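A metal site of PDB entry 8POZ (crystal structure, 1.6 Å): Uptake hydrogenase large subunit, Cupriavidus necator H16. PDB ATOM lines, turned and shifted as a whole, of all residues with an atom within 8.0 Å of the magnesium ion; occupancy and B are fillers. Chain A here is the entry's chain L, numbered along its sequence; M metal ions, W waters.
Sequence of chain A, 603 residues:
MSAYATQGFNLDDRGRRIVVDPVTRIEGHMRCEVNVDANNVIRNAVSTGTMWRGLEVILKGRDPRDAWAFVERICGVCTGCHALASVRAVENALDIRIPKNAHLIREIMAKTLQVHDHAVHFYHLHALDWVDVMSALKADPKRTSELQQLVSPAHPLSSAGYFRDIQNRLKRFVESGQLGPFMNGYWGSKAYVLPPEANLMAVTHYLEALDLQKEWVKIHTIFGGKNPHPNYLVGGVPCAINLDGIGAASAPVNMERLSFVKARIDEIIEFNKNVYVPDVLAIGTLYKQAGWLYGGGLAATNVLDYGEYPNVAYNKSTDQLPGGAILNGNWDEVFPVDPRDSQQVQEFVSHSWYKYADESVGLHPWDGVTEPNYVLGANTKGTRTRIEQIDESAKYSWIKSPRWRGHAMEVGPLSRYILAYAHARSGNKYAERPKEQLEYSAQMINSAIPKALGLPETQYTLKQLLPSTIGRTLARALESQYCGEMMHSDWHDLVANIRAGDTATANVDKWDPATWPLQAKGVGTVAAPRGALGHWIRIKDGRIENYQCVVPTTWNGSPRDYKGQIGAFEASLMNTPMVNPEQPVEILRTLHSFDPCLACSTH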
ATOM      1  N   TRP A  52       8.822   7.814  -9.541  1.00  0.00           N
ATOM      2  CA  TRP A  52       9.076   6.690 -10.445  1.00  0.00           C
ATOM      3  C   TRP A  52       7.754   6.164 -10.979  1.00  0.00           C
ATOM      4  O   TRP A  52       6.774   6.119 -10.237  1.00  0.00           O
ATOM      5  CB  TRP A  52       9.831   5.574  -9.724  1.00  0.00           C
ATOM      6  CG  TRP A  52      10.097   4.370 -10.587  1.00  0.00           C
ATOM      7  CD1 TRP A  52      10.871   4.318 -11.722  1.00  0.00           C
ATOM      8  CD2 TRP A  52       9.599   3.050 -10.386  1.00  0.00           C
ATOM      9  NE1 TRP A  52      10.870   3.040 -12.228  1.00  0.00           N
ATOM     10  CE2 TRP A  52      10.097   2.242 -11.429  1.00  0.00           C
ATOM     11  CE3 TRP A  52       8.758   2.466  -9.416  1.00  0.00           C
ATOM     12  CZ2 TRP A  52       9.797   0.881 -11.530  1.00  0.00           C
ATOM     13  CZ3 TRP A  52       8.467   1.123  -9.520  1.00  0.00           C
ATOM     14  CH2 TRP A  52       8.980   0.341 -10.567  1.00  0.00           C
ATOM     15  N   GLU A  56       9.841   0.959 -18.100  1.00  0.00           N
ATOM     16  CA  GLU A  56      10.643  -0.176 -18.535  1.00  0.00           C
ATOM     17  C   GLU A  56       9.936  -1.500 -18.210  1.00  0.00           C
ATOM     18  O   GLU A  56       9.961  -2.435 -19.013  1.00  0.00           O
ATOM     19  CB  GLU A  56      12.035  -0.104 -17.920  1.00  0.00           C
ATOM     20  CG  GLU A  56      12.833   1.081 -18.440  1.00  0.00           C
ATOM     21  CD  GLU A  56      13.971   1.489 -17.539  1.00  0.00           C
ATOM     22  OE1 GLU A  56      13.870   1.284 -16.316  1.00  0.00           O
ATOM     23  OE2 GLU A  56      14.972   2.052 -18.063  1.00  0.00           O
ATOM     24  N   ILE A  74       7.069   9.263 -21.306  1.00  0.00           N
ATOM     25  CA  ILE A  74       8.072   9.521 -20.289  1.00  0.00           C
ATOM     26  C   ILE A  74       8.101  11.018 -19.983  1.00  0.00           C
ATOM     27  O   ILE A  74       8.275  11.411 -18.837  1.00  0.00           O
ATOM     28  CB  ILE A  74       9.475   9.023 -20.708  1.00  0.00           C
ATOM     29  CG1 ILE A  74       9.522   7.490 -20.675  1.00  0.00           C
ATOM     30  CG2 ILE A  74      10.563   9.598 -19.807  1.00  0.00           C
ATOM     31  CD1 ILE A  74      10.744   6.895 -21.330  1.00  0.00           C
ATOM     32  N   GLU A 347      24.879   1.214 -15.750  1.00  0.00           N
ATOM     33  CA  GLU A 347      24.133   1.853 -14.673  1.00  0.00           C
ATOM     34  C   GLU A 347      24.279   1.097 -13.366  1.00  0.00           C
ATOM     35  O   GLU A 347      24.099  -0.124 -13.320  1.00  0.00           O
ATOM     36  CB  GLU A 347      22.645   1.968 -15.018  1.00  0.00           C
ATOM     37  CG  GLU A 347      22.347   2.953 -16.134  1.00  0.00           C
ATOM     38  CD  GLU A 347      20.860   3.048 -16.381  1.00  0.00           C
ATOM     39  OE1 GLU A 347      20.270   2.029 -16.805  1.00  0.00           O
ATOM     40  OE2 GLU A 347      20.305   4.140 -16.162  1.00  0.00           O
ATOM     41  N   TYR A 354      16.525   0.708  -6.187  1.00  0.00           N
ATOM     42  CA  TYR A 354      16.367  -0.484  -6.999  1.00  0.00           C
ATOM     43  C   TYR A 354      17.252  -1.582  -6.440  1.00  0.00           C
ATOM     44  O   TYR A 354      18.064  -1.348  -5.523  1.00  0.00           O
ATOM     45  CB  TYR A 354      16.771  -0.218  -8.452  1.00  0.00           C
ATOM     46  CG  TYR A 354      16.022   0.921  -9.073  1.00  0.00           C
ATOM     47  CD1 TYR A 354      14.729   0.755  -9.568  1.00  0.00           C
ATOM     48  CD2 TYR A 354      16.586   2.190  -9.144  1.00  0.00           C
ATOM     49  CE1 TYR A 354      14.028   1.808 -10.121  1.00  0.00           C
ATOM     50  CE2 TYR A 354      15.898   3.247  -9.703  1.00  0.00           C
ATOM     51  CZ  TYR A 354      14.619   3.051 -10.187  1.00  0.00           C
ATOM     52  OH  TYR A 354      13.914   4.096 -10.739  1.00  0.00           O
ATOM     53  N   PRO A 365      22.761  -1.370 -20.578  1.00  0.00           N
ATOM     54  CA  PRO A 365      21.286  -1.405 -20.656  1.00  0.00           C
ATOM     55  C   PRO A 365      20.652  -2.587 -21.390  1.00  0.00           C
ATOM     56  O   PRO A 365      19.483  -2.891 -21.134  1.00  0.00           O
ATOM     57  CB  PRO A 365      20.944  -0.087 -21.342  1.00  0.00           C
ATOM     58  CG  PRO A 365      22.105   0.804 -21.045  1.00  0.00           C
ATOM     59  CD  PRO A 365      23.289  -0.109 -21.125  1.00  0.00           C
ATOM     60  N   GLY A 368      20.042  -4.575 -18.526  1.00  0.00           N
ATOM     61  CA  GLY A 368      19.534  -3.756 -17.444  1.00  0.00           C
ATOM     62  C   GLY A 368      18.369  -4.408 -16.738  1.00  0.00           C
ATOM     63  O   GLY A 368      17.650  -5.228 -17.310  1.00  0.00           O
ATOM     64  N   VAL A 369      18.206  -4.029 -15.473  1.00  0.00           N
ATOM     65  CA  VAL A 369      17.199  -4.591 -14.588  1.00  0.00           C
ATOM     66  C   VAL A 369      16.549  -3.421 -13.831  1.00  0.00           C
ATOM     67  O   VAL A 369      17.250  -2.524 -13.353  1.00  0.00           O
ATOM     68  CB  VAL A 369      17.848  -5.595 -13.600  1.00  0.00           C
ATOM     69  CG1 VAL A 369      16.866  -6.041 -12.546  1.00  0.00           C
ATOM     70  CG2 VAL A 369      18.414  -6.789 -14.363  1.00  0.00           C
ATOM     71  N   THR A 370      15.223  -3.433 -13.744  1.00  0.00           N
ATOM     72  CA  THR A 370      14.486  -2.392 -13.017  1.00  0.00           C
ATOM     73  C   THR A 370      13.502  -3.031 -12.028  1.00  0.00           C
ATOM     74  O   THR A 370      12.327  -3.235 -12.340  1.00  0.00           O
ATOM     75  CB  THR A 370      13.750  -1.427 -13.977  1.00  0.00           C
ATOM     76  OG1 THR A 370      14.691  -0.921 -14.937  1.00  0.00           O
ATOM     77  CG2 THR A 370      13.145  -0.247 -13.219  1.00  0.00           C
ATOM     78  N   TRP A 398      15.273   7.753  -6.847  1.00  0.00           N
ATOM     79  CA  TRP A 398      14.694   6.909  -7.893  1.00  0.00           C
ATOM     80  C   TRP A 398      15.501   6.939  -9.202  1.00  0.00           C
ATOM     81  O   TRP A 398      15.172   6.236 -10.153  1.00  0.00           O
ATOM     82  CB  TRP A 398      13.236   7.295  -8.166  1.00  0.00           C
ATOM     83  CG  TRP A 398      12.316   6.842  -7.086  1.00  0.00           C
ATOM     84  CD1 TRP A 398      11.654   7.615  -6.180  1.00  0.00           C
ATOM     85  CD2 TRP A 398      11.950   5.485  -6.797  1.00  0.00           C
ATOM     86  NE1 TRP A 398      10.901   6.836  -5.343  1.00  0.00           N
ATOM     87  CE2 TRP A 398      11.061   5.514  -5.699  1.00  0.00           C
ATOM     88  CE3 TRP A 398      12.282   4.244  -7.361  1.00  0.00           C
ATOM     89  CZ2 TRP A 398      10.502   4.363  -5.146  1.00  0.00           C
ATOM     90  CZ3 TRP A 398      11.730   3.089  -6.812  1.00  0.00           C
ATOM     91  CH2 TRP A 398      10.841   3.163  -5.720  1.00  0.00           C
ATOM     92  N   ILE A 399      16.567   7.746  -9.259  1.00  0.00           N
ATOM     93  CA  ILE A 399      17.413   7.832 -10.446  1.00  0.00           C
ATOM     94  C   ILE A 399      18.542   6.810 -10.311  1.00  0.00           C
ATOM     95  O   ILE A 399      19.218   6.755  -9.283  1.00  0.00           O
ATOM     96  CB  ILE A 399      18.004   9.257 -10.602  1.00  0.00           C
ATOM     97  CG1 ILE A 399      16.889  10.319 -10.572  1.00  0.00           C
ATOM     98  CG2 ILE A 399      18.787   9.383 -11.900  1.00  0.00           C
ATOM     99  CD1 ILE A 399      17.389  11.744 -10.538  1.00  0.00           C
ATOM    100  N   LYS A 400      18.741   5.997 -11.343  1.00  0.00           N
ATOM    101  CA  LYS A 400      19.915   5.113 -11.426  1.00  0.00           C
ATOM    102  C   LYS A 400      21.189   5.941 -11.650  1.00  0.00           C
ATOM    103  O   LYS A 400      21.127   7.132 -11.928  1.00  0.00           O
ATOM    104  CB  LYS A 400      19.752   4.103 -12.572  1.00  0.00           C
ATOM    105  CG  LYS A 400      18.609   3.114 -12.398  1.00  0.00           C
ATOM    106  CD  LYS A 400      18.680   2.022 -13.455  1.00  0.00           C
ATOM    107  CE  LYS A 400      17.558   1.012 -13.338  1.00  0.00           C
ATOM    108  NZ  LYS A 400      17.435   0.166 -14.551  1.00  0.00           N
ATOM    109  N   PRO A 402      24.182   6.245 -14.084  1.00  0.00           N
ATOM    110  CA  PRO A 402      24.901   5.876 -15.307  1.00  0.00           C
ATOM    111  C   PRO A 402      26.334   6.381 -15.254  1.00  0.00           C
ATOM    112  O   PRO A 402      26.577   7.486 -14.774  1.00  0.00           O
ATOM    113  CB  PRO A 402      24.128   6.594 -16.423  1.00  0.00           C
ATOM    114  CG  PRO A 402      22.933   7.209 -15.768  1.00  0.00           C
ATOM    115  CD  PRO A 402      23.310   7.395 -14.330  1.00  0.00           C
ATOM    116  N   GLY A 534      19.514   7.338 -24.736  1.00  0.00           N
ATOM    117  CA  GLY A 534      19.586   6.023 -25.372  1.00  0.00           C
ATOM    118  C   GLY A 534      18.450   5.117 -24.933  1.00  0.00           C
ATOM    119  O   GLY A 534      18.074   5.116 -23.754  1.00  0.00           O
ATOM    120  N   TRP A 536      17.545   0.977 -25.320  1.00  0.00           N
ATOM    121  CA  TRP A 536      18.101  -0.331 -25.666  1.00  0.00           C
ATOM    122  C   TRP A 536      16.991  -1.366 -25.592  1.00  0.00           C
ATOM    123  O   TRP A 536      16.358  -1.523 -24.551  1.00  0.00           O
ATOM    124  CB  TRP A 536      19.202  -0.700 -24.692  1.00  0.00           C
ATOM    125  CG  TRP A 536      20.524   0.013 -24.886  1.00  0.00           C
ATOM    126  CD1 TRP A 536      21.620  -0.486 -25.524  1.00  0.00           C
ATOM    127  CD2 TRP A 536      20.888   1.325 -24.429  1.00  0.00           C
ATOM    128  NE1 TRP A 536      22.644   0.417 -25.483  1.00  0.00           N
ATOM    129  CE2 TRP A 536      22.229   1.547 -24.823  1.00  0.00           C
ATOM    130  CE3 TRP A 536      20.214   2.339 -23.724  1.00  0.00           C
ATOM    131  CZ2 TRP A 536      22.915   2.733 -24.539  1.00  0.00           C
ATOM    132  CZ3 TRP A 536      20.912   3.520 -23.435  1.00  0.00           C
ATOM    133  CH2 TRP A 536      22.244   3.699 -23.842  1.00  0.00           C
ATOM    134  N   TYR A 547      13.528  -3.665 -22.299  1.00  0.00           N
ATOM    135  CA  TYR A 547      13.539  -2.294 -22.793  1.00  0.00           C
ATOM    136  C   TYR A 547      14.094  -1.435 -21.666  1.00  0.00           C
ATOM    137  O   TYR A 547      13.500  -1.355 -20.594  1.00  0.00           O
ATOM    138  CB  TYR A 547      12.150  -1.844 -23.226  1.00  0.00           C
ATOM    139  CG  TYR A 547      12.133  -0.669 -24.200  1.00  0.00           C
ATOM    140  CD1 TYR A 547      12.579   0.596 -23.823  1.00  0.00           C
ATOM    141  CD2 TYR A 547      11.675  -0.848 -25.508  1.00  0.00           C
ATOM    142  CE1 TYR A 547      12.571   1.661 -24.724  1.00  0.00           C
ATOM    143  CE2 TYR A 547      11.663   0.209 -26.408  1.00  0.00           C
ATOM    144  CZ  TYR A 547      12.104   1.455 -26.019  1.00  0.00           C
ATOM    145  OH  TYR A 547      12.080   2.482 -26.929  1.00  0.00           O
ATOM    146  N   GLN A 548      15.250  -0.821 -21.902  1.00  0.00           N
ATOM    147  CA  GLN A 548      15.920   0.001 -20.903  1.00  0.00           C
ATOM    148  C   GLN A 548      16.262   1.358 -21.494  1.00  0.00           C
ATOM    149  O   GLN A 548      16.789   1.459 -22.612  1.00  0.00           O
ATOM    150  CB  GLN A 548      17.178  -0.703 -20.413  1.00  0.00           C
ATOM    151  CG  GLN A 548      16.873  -1.938 -19.569  1.00  0.00           C
ATOM    152  CD  GLN A 548      16.410  -1.601 -18.162  1.00  0.00           C
ATOM    153  OE1 GLN A 548      16.879  -0.638 -17.563  1.00  0.00           O
ATOM    154  NE2 GLN A 548      15.492  -2.394 -17.626  1.00  0.00           N
ATOM    155  N   CYS A 549      15.933   2.397 -20.742  1.00  0.00           N
ATOM    156  CA  CYS A 549      16.222   3.767 -21.137  1.00  0.00           C
ATOM    157  C   CYS A 549      17.254   4.344 -20.198  1.00  0.00           C
ATOM    158  O   CYS A 549      17.166   4.143 -18.981  1.00  0.00           O
ATOM    159  CB  CYS A 549      14.956   4.623 -21.045  1.00  0.00           C
ATOM    160  SG  CYS A 549      13.553   4.012 -21.975  1.00  0.00           S
ATOM    161  N   VAL A 550      18.224   5.045 -20.769  1.00  0.00           N
ATOM    162  CA  VAL A 550      19.143   5.865 -20.003  1.00  0.00           C
ATOM    163  C   VAL A 550      19.040   7.259 -20.608  1.00  0.00           C
ATOM    164  O   VAL A 550      19.352   7.469 -21.788  1.00  0.00           O
ATOM    165  CB  VAL A 550      20.600   5.355 -20.081  1.00  0.00           C
ATOM    166  CG1 VAL A 550      21.494   6.137 -19.129  1.00  0.00           C
ATOM    167  CG2 VAL A 550      20.645   3.856 -19.763  1.00  0.00           C
ATOM    168  N   VAL A 551      18.611   8.202 -19.784  1.00  0.00           N
ATOM    169  CA  VAL A 551      18.091   9.484 -20.231  1.00  0.00           C
ATOM    170  C   VAL A 551      19.048  10.586 -19.743  1.00  0.00           C
ATOM    171  O   VAL A 551      19.807  10.355 -18.809  1.00  0.00           O
ATOM    172  CB  VAL A 551      16.642   9.599 -19.689  1.00  0.00           C
ATOM    173  CG1 VAL A 551      15.914  10.808 -20.233  1.00  0.00           C
ATOM    174  CG2 VAL A 551      15.841   8.341 -20.026  1.00  0.00           C
ATOM    175  N   THR A 554      19.070  11.312 -16.166  1.00  0.00           N
ATOM    176  CA  THR A 554      19.575  10.142 -15.430  1.00  0.00           C
ATOM    177  C   THR A 554      21.080  10.312 -15.194  1.00  0.00           C
ATOM    178  O   THR A 554      21.551  10.130 -14.080  1.00  0.00           O
ATOM    179  CB  THR A 554      19.325   8.788 -16.126  1.00  0.00           C
ATOM    180  OG1 THR A 554      17.996   8.749 -16.667  1.00  0.00           O
ATOM    181  CG2 THR A 554      19.504   7.629 -15.140  1.00  0.00           C
ATOM    182  N   CYS A 600      11.737  12.267 -16.914  1.00  0.00           N
ATOM    183  CA  CYS A 600      12.715  11.657 -17.799  1.00  0.00           C
ATOM    184  C   CYS A 600      13.749  10.826 -17.070  1.00  0.00           C
ATOM    185  O   CYS A 600      14.061   9.701 -17.476  1.00  0.00           O
ATOM    186  CB  CYS A 600      13.468  12.734 -18.578  1.00  0.00           C
ATOM    187  SG  CYS A 600      12.825  12.949 -20.243  1.00  0.00           S
ATOM    188  N   SER A 601      14.293  11.383 -15.994  1.00  0.00           N
ATOM    189  CA  SER A 601      15.419  10.772 -15.306  1.00  0.00           C
ATOM    190  C   SER A 601      15.083   9.397 -14.732  1.00  0.00           C
ATOM    191  O   SER A 601      15.940   8.527 -14.670  1.00  0.00           O
ATOM    192  CB  SER A 601      15.957  11.683 -14.199  1.00  0.00           C
ATOM    193  OG  SER A 601      15.115  11.704 -13.057  1.00  0.00           O
ATOM    194  N   THR A 602      13.819   9.223 -14.347  1.00  0.00           N
ATOM    195  CA  THR A 602      13.361   8.029 -13.636  1.00  0.00           C
ATOM    196  C   THR A 602      12.495   7.108 -14.495  1.00  0.00           C
ATOM    197  O   THR A 602      12.558   5.884 -14.344  1.00  0.00           O
ATOM    198  CB  THR A 602      12.574   8.442 -12.375  1.00  0.00           C
ATOM    199  OG1 THR A 602      11.473   9.285 -12.746  1.00  0.00           O
ATOM    200  CG2 THR A 602      13.483   9.185 -11.401  1.00  0.00           C
ATOM    201  N   HIS A 603      11.711   7.693 -15.387  1.00  0.00           N
ATOM    202  CA  HIS A 603      10.841   6.938 -16.303  1.00  0.00           C
ATOM    203  C   HIS A 603      10.167   5.731 -15.633  1.00  0.00           C
ATOM    204  O   HIS A 603      10.126   4.621 -16.168  1.00  0.00           O
ATOM    205  CB  HIS A 603      11.577   6.569 -17.612  1.00  0.00           C
ATOM    206  CG  HIS A 603      12.982   6.095 -17.425  1.00  0.00           C
ATOM    207  ND1 HIS A 603      14.041   6.954 -17.249  1.00  0.00           N
ATOM    208  CD2 HIS A 603      13.504   4.839 -17.401  1.00  0.00           C
ATOM    209  CE1 HIS A 603      15.162   6.258 -17.128  1.00  0.00           C
ATOM    210  NE2 HIS A 603      14.857   4.972 -17.207  1.00  0.00           N
ATOM    211  OXT HIS A 603       9.617   5.873 -14.531  1.00  0.00           O
HETATM  212 MG    MG M   1      16.433   3.360 -17.125  1.00  0.00          MG
HETATM  213  O   HOH W   1      17.777   1.775 -17.250  1.00  0.00           O
HETATM  214  O   HOH W   2      15.748   2.796 -15.245  1.00  0.00           O
HETATM  215  O   HOH W   3      17.762   4.616 -16.173  1.00  0.00           O
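The side-chain carboxylate of Glu 56 sits close to the side-chain amide oxygen of Gln 548 (3.3 Å).
The side-chain carboxylate of Glu 56 is in hydrogen-bond range of the side-chain hydroxyl of Thr 370, at 2.7 Å.
A ring nitrogen (ND1) of His 603 lies within hydrogen-bond range of the backbone carbonyl oxygen (O) of Cys 600 (2.8 Å).
Three residues have an atom within 4 Å of the magnesium ion: Glu 56, Cys 549 and His 603.
The nearest printed residue that does not touch the magnesium ion is Gln 548 (4.05 Å).
Water W3 is bound to the magnesium ion (2.1 Å).
Water W2 binds the magnesium ion (2.1 Å).
The magnesium ion is bound by water W1.
O of Cys 549 is bound to the magnesium ion, at 2.1 Å.
The side-chain carboxylate (OE2) of Glu 56 is bound to the magnesium ion, 2.2 Å away.
NE2 of His 603 is bound to the magnesium ion.
Water W1 lies within hydrogen-bond range of OE1 of Glu 347, OE1 of Gln 548 and NZ of Lys 400.
Water W2 lies within hydrogen-bond range of OE1 of Glu 56 and NZ of Lys 400.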
